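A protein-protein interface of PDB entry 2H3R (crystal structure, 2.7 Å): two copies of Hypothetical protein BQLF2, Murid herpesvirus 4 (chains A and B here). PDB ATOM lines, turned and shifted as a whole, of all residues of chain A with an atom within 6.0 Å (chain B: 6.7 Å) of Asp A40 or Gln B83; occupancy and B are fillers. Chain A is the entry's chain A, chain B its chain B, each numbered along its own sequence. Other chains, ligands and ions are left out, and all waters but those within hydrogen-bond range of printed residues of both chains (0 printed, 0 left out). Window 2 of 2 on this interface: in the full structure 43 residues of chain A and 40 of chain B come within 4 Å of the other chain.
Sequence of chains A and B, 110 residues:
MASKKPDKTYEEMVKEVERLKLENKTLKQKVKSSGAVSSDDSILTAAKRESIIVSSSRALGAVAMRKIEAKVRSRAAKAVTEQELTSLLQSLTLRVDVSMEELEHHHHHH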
ATOM      1  N   LYS A  21      -1.894  23.720 -16.507  1.00  0.00           N
ATOM      2  CA  LYS A  21      -0.560  24.298 -16.675  1.00  0.00           C
ATOM      3  C   LYS A  21      -0.367  24.715 -18.134  1.00  0.00           C
ATOM      4  O   LYS A  21       0.366  25.664 -18.448  1.00  0.00           O
ATOM      5  CB  LYS A  21       0.532  23.300 -16.241  1.00  0.00           C
ATOM      6  CG  LYS A  21       0.512  22.972 -14.736  1.00  0.00           C
ATOM      7  CD  LYS A  21       1.688  22.092 -14.296  1.00  0.00           C
ATOM      8  CE  LYS A  21       1.733  21.914 -12.766  1.00  0.00           C
ATOM      9  NZ  LYS A  21       2.865  21.056 -12.285  1.00  0.00           N
ATOM     10  N   ASN A  24      -2.544  27.574 -18.609  1.00  0.00           N
ATOM     11  CA  ASN A  24      -1.884  28.647 -17.870  1.00  0.00           C
ATOM     12  C   ASN A  24      -0.760  29.251 -18.698  1.00  0.00           C
ATOM     13  O   ASN A  24      -0.471  30.436 -18.583  1.00  0.00           O
ATOM     14  CB  ASN A  24      -1.320  28.137 -16.540  1.00  0.00           C
ATOM     15  CG  ASN A  24      -0.453  29.175 -15.837  1.00  0.00           C
ATOM     16  OD1 ASN A  24       0.714  29.370 -16.182  1.00  0.00           O
ATOM     17  ND2 ASN A  24      -1.031  29.856 -14.853  1.00  0.00           N
ATOM     18  N   LYS A  25      -0.118  28.439 -19.527  1.00  0.00           N
ATOM     19  CA  LYS A  25       0.955  28.953 -20.360  1.00  0.00           C
ATOM     20  C   LYS A  25       0.325  29.819 -21.443  1.00  0.00           C
ATOM     21  O   LYS A  25       0.630  31.003 -21.545  1.00  0.00           O
ATOM     22  CB  LYS A  25       1.765  27.810 -20.987  1.00  0.00           C
ATOM     23  CG  LYS A  25       3.032  28.306 -21.685  1.00  0.00           C
ATOM     24  CD  LYS A  25       3.976  27.180 -22.099  1.00  0.00           C
ATOM     25  CE  LYS A  25       3.445  26.389 -23.284  1.00  0.00           C
ATOM     26  NZ  LYS A  25       4.461  25.421 -23.778  1.00  0.00           N
ATOM     27  N   LYS A  28      -0.266  33.075 -20.363  1.00  0.00           N
ATOM     28  CA  LYS A  28       0.932  33.888 -20.127  1.00  0.00           C
ATOM     29  C   LYS A  28       1.523  34.256 -21.491  1.00  0.00           C
ATOM     30  O   LYS A  28       2.194  35.274 -21.651  1.00  0.00           O
ATOM     31  CB  LYS A  28       1.977  33.114 -19.311  1.00  0.00           C
ATOM     32  CG  LYS A  28       1.639  32.882 -17.838  1.00  0.00           C
ATOM     33  CD  LYS A  28       2.791  32.150 -17.135  1.00  0.00           C
ATOM     34  CE  LYS A  28       2.701  32.212 -15.608  1.00  0.00           C
ATOM     35  NZ  LYS A  28       1.526  31.467 -15.047  1.00  0.00           N
ATOM     36  N   GLN A  29       1.268  33.412 -22.483  1.00  0.00           N
ATOM     37  CA  GLN A  29       1.766  33.664 -23.821  1.00  0.00           C
ATOM     38  C   GLN A  29       0.942  34.803 -24.397  1.00  0.00           C
ATOM     39  O   GLN A  29       1.466  35.666 -25.089  1.00  0.00           O
ATOM     40  CB  GLN A  29       1.634  32.405 -24.680  1.00  0.00           C
ATOM     41  CG  GLN A  29       2.924  32.008 -25.392  1.00  0.00           C
ATOM     42  CD  GLN A  29       3.098  30.500 -25.498  1.00  0.00           C
ATOM     43  OE1 GLN A  29       2.244  29.797 -26.046  1.00  0.00           O
ATOM     44  NE2 GLN A  29       4.209  29.997 -24.966  1.00  0.00           N
ATOM     45  N   SER A  39       6.055  36.323 -20.805  1.00  0.00           N
ATOM     46  CA  SER A  39       7.287  36.180 -20.039  1.00  0.00           C
ATOM     47  C   SER A  39       7.027  35.967 -18.557  1.00  0.00           C
ATOM     48  O   SER A  39       7.197  36.884 -17.753  1.00  0.00           O
ATOM     49  CB  SER A  39       8.174  37.413 -20.215  1.00  0.00           C
ATOM     50  OG  SER A  39       9.267  37.374 -19.313  1.00  0.00           O
ATOM     51  N   ASP A  40       6.608  34.760 -18.200  1.00  0.00           N
ATOM     52  CA  ASP A  40       6.341  34.433 -16.805  1.00  0.00           C
ATOM     53  C   ASP A  40       6.605  32.946 -16.623  1.00  0.00           C
ATOM     54  O   ASP A  40       5.720  32.181 -16.238  1.00  0.00           O
ATOM     55  CB  ASP A  40       4.889  34.769 -16.443  1.00  0.00           C
ATOM     56  CG  ASP A  40       4.667  34.885 -14.939  1.00  0.00           C
ATOM     57  OD1 ASP A  40       5.011  33.932 -14.207  1.00  0.00           O
ATOM     58  OD2 ASP A  40       4.144  35.933 -14.490  1.00  0.00           O
ATOM     59  N   ASP A  41       7.836  32.546 -16.920  1.00  0.00           N
ATOM     60  CA  ASP A  41       8.253  31.160 -16.805  1.00  0.00           C
ATOM     61  C   ASP A  41       9.376  31.018 -15.786  1.00  0.00           C
ATOM     62  O   ASP A  41      10.551  31.231 -16.087  1.00  0.00           O
ATOM     63  CB  ASP A  41       8.710  30.645 -18.168  1.00  0.00           C
ATOM     64  CG  ASP A  41       9.245  29.236 -18.104  1.00  0.00           C
ATOM     65  OD1 ASP A  41       8.647  28.414 -17.383  1.00  0.00           O
ATOM     66  OD2 ASP A  41      10.254  28.950 -18.786  1.00  0.00           O
ATOM     67  N   SER A  42       8.993  30.646 -14.574  1.00  0.00           N
ATOM     68  CA  SER A  42       9.934  30.468 -13.479  1.00  0.00           C
ATOM     69  C   SER A  42      10.780  29.210 -13.607  1.00  0.00           C
ATOM     70  O   SER A  42      10.438  28.272 -14.326  1.00  0.00           O
ATOM     71  CB  SER A  42       9.162  30.405 -12.166  1.00  0.00           C
ATOM     72  OG  SER A  42       8.184  31.426 -12.117  1.00  0.00           O
ATOM     73  N   THR B  81      12.856  24.886 -16.357  1.00  0.00           N
ATOM     74  CA  THR B  81      11.760  25.821 -16.126  1.00  0.00           C
ATOM     75  C   THR B  81      10.460  25.026 -16.048  1.00  0.00           C
ATOM     76  O   THR B  81      10.417  23.859 -16.437  1.00  0.00           O
ATOM     77  CB  THR B  81      11.632  26.872 -17.276  1.00  0.00           C
ATOM     78  OG1 THR B  81      11.202  26.220 -18.484  1.00  0.00           O
ATOM     79  CG2 THR B  81      12.966  27.578 -17.521  1.00  0.00           C
ATOM     80  N   GLU B  82       9.406  25.661 -15.550  1.00  0.00           N
ATOM     81  CA  GLU B  82       8.108  25.012 -15.403  1.00  0.00           C
ATOM     82  C   GLU B  82       7.323  24.875 -16.702  1.00  0.00           C
ATOM     83  O   GLU B  82       6.547  23.933 -16.864  1.00  0.00           O
ATOM     84  CB  GLU B  82       7.268  25.758 -14.365  1.00  0.00           C
ATOM     85  CG  GLU B  82       7.809  25.618 -12.957  1.00  0.00           C
ATOM     86  CD  GLU B  82       6.992  26.373 -11.932  1.00  0.00           C
ATOM     87  OE1 GLU B  82       6.973  27.620 -11.984  1.00  0.00           O
ATOM     88  OE2 GLU B  82       6.369  25.715 -11.072  1.00  0.00           O
ATOM     89  N   GLN B  83       7.508  25.804 -17.631  1.00  0.00           N
ATOM     90  CA  GLN B  83       6.797  25.705 -18.901  1.00  0.00           C
ATOM     91  C   GLN B  83       7.463  24.640 -19.773  1.00  0.00           C
ATOM     92  O   GLN B  83       6.797  23.894 -20.488  1.00  0.00           O
ATOM     93  CB  GLN B  83       6.761  27.069 -19.608  1.00  0.00           C
ATOM     94  CG  GLN B  83       5.589  27.952 -19.151  1.00  0.00           C
ATOM     95  CD  GLN B  83       5.625  29.377 -19.707  1.00  0.00           C
ATOM     96  OE1 GLN B  83       5.662  29.592 -20.923  1.00  0.00           O
ATOM     97  NE2 GLN B  83       5.599  30.359 -18.809  1.00  0.00           N
ATOM     98  N   GLU B  84       8.783  24.552 -19.674  1.00  0.00           N
ATOM     99  CA  GLU B  84       9.549  23.574 -20.437  1.00  0.00           C
ATOM    100  C   GLU B  84       9.138  22.152 -20.059  1.00  0.00           C
ATOM    101  O   GLU B  84       9.076  21.263 -20.911  1.00  0.00           O
ATOM    102  CB  GLU B  84      11.036  23.771 -20.156  1.00  0.00           C
ATOM    103  CG  GLU B  84      11.907  23.789 -21.380  1.00  0.00           C
ATOM    104  CD  GLU B  84      13.323  24.199 -21.050  1.00  0.00           C
ATOM    105  OE1 GLU B  84      13.958  23.516 -20.214  1.00  0.00           O
ATOM    106  OE2 GLU B  84      13.805  25.205 -21.615  1.00  0.00           O
ATOM    107  N   LEU B  85       8.855  21.942 -18.776  1.00  0.00           N
ATOM    108  CA  LEU B  85       8.456  20.629 -18.301  1.00  0.00           C
ATOM    109  C   LEU B  85       6.966  20.397 -18.571  1.00  0.00           C
ATOM    110  O   LEU B  85       6.514  19.255 -18.678  1.00  0.00           O
ATOM    111  CB  LEU B  85       8.777  20.488 -16.808  1.00  0.00           C
ATOM    112  CG  LEU B  85       8.834  19.054 -16.257  1.00  0.00           C
ATOM    113  CD1 LEU B  85       9.796  18.213 -17.073  1.00  0.00           C
ATOM    114  CD2 LEU B  85       9.266  19.082 -14.803  1.00  0.00           C
ATOM    115  N   THR B  86       6.204  21.481 -18.684  1.00  0.00           N
ATOM    116  CA  THR B  86       4.785  21.367 -18.985  1.00  0.00           C
ATOM    117  C   THR B  86       4.682  20.961 -20.448  1.00  0.00           C
ATOM    118  O   THR B  86       3.973  20.019 -20.797  1.00  0.00           O
ATOM    119  CB  THR B  86       4.046  22.694 -18.770  1.00  0.00           C
ATOM    120  OG1 THR B  86       3.898  22.926 -17.368  1.00  0.00           O
ATOM    121  CG2 THR B  86       2.659  22.651 -19.415  1.00  0.00           C
ATOM    122  N   SER B  87       5.396  21.676 -21.308  1.00  0.00           N
ATOM    123  CA  SER B  87       5.394  21.341 -22.719  1.00  0.00           C
ATOM    124  C   SER B  87       5.784  19.858 -22.865  1.00  0.00           C
ATOM    125  O   SER B  87       5.043  19.058 -23.446  1.00  0.00           O
ATOM    126  CB  SER B  87       6.393  22.233 -23.452  1.00  0.00           C
ATOM    127  OG  SER B  87       6.920  21.565 -24.585  1.00  0.00           O
ATOM    128  N   LEU B  88       6.943  19.509 -22.303  1.00  0.00           N
ATOM    129  CA  LEU B  88       7.489  18.149 -22.339  1.00  0.00           C
ATOM    130  C   LEU B  88       6.541  17.049 -21.861  1.00  0.00           C
ATOM    131  O   LEU B  88       6.445  15.987 -22.484  1.00  0.00           O
ATOM    132  CB  LEU B  88       8.779  18.107 -21.508  1.00  0.00           C
ATOM    133  CG  LEU B  88       9.550  16.801 -21.254  1.00  0.00           C
ATOM    134  CD1 LEU B  88      10.919  17.163 -20.697  1.00  0.00           C
ATOM    135  CD2 LEU B  88       8.819  15.892 -20.271  1.00  0.00           C
ATOM    136  N   LEU B  89       5.849  17.295 -20.754  1.00  0.00           N
ATOM    137  CA  LEU B  89       4.929  16.311 -20.183  1.00  0.00           C
ATOM    138  C   LEU B  89       3.555  16.289 -20.820  1.00  0.00           C
ATOM    139  O   LEU B  89       2.702  15.491 -20.437  1.00  0.00           O
ATOM    140  CB  LEU B  89       4.783  16.548 -18.682  1.00  0.00           C
ATOM    141  CG  LEU B  89       5.978  16.052 -17.882  1.00  0.00           C
ATOM    142  CD1 LEU B  89       5.984  16.648 -16.495  1.00  0.00           C
ATOM    143  CD2 LEU B  89       5.918  14.539 -17.845  1.00  0.00           C
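Printed residues of chain B that touch a printed residue of chain A: Thr B81, Glu B82, Gln B83, Thr B86 and Ser B87.
No position is printed for both chains.
Of the 10 pairs that touch across the chains among the printed residues, none has its exchanged pair printed and touching as well.
NZ of Lys A28 is in hydrogen-bond range of OD1 of Asn A24, 2.5 Å away.
The side-chain hydroxyl of Thr B81 lies close to the backbone NH of Glu B84 (3.2 Å).
The side-chain hydroxyl (OG1) of Thr B86 sits at hydrogen-bond distance from the backbone carbonyl oxygen (O) of Glu B82 (2.9 Å).
Asn A24 touches none of the printed residues of chain B.
Of the printed residues of chain B, Lys A25 touches Gln B83 (3.0 Å) and Ser B87 (3.7 Å).
Asp A40 touches just one residue of chain B: Gln B83 (3.2 Å).
Printed residues of chain A within 4 Å of Thr B81: Asp A41 (2.9 Å) and Ser A42 (3.3 Å).
Leu B85 touches none of the printed residues of chain A.
Of the printed residues of chain A, Thr B86 touches Lys A21.
Of the printed residues of chain A, Ser B87 touches Lys A25 (3.7 Å).
The nearest residue of chain A that does not touch Gln B83 is Gln A29 (4.3 Å).
NE2 of Gln B83 lies within hydrogen-bond range of O of Asp A40, at 3.2 Å.
OD2 of Asp A41 is in hydrogen-bond range of OG1 of Thr B81, 2.9 Å away.
The side-chain carboxylate of Asp A41 is in hydrogen-bond range of the backbone NH of Glu B82 (3.4 Å).
The backbone NH (N) of Gln B83 is in hydrogen-bond range of the side-chain carboxylate (OD1) of Asp A41, at 2.9 Å.
The backbone carbonyl oxygen of Ser A42 sits at hydrogen-bond distance from the backbone NH of Glu B82, at 3.1 Å.
Among the printed residues, pairs that only touch across the chains: Lys A25 with Gln B83 (3.0 Å), Ser A42 with Thr B81 (3.3 Å), Lys A21 with Thr B86 (3.6 Å), Lys A28 with Gln B83 (3.7 Å) and Lys A25 with Ser B87 (3.7 Å).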
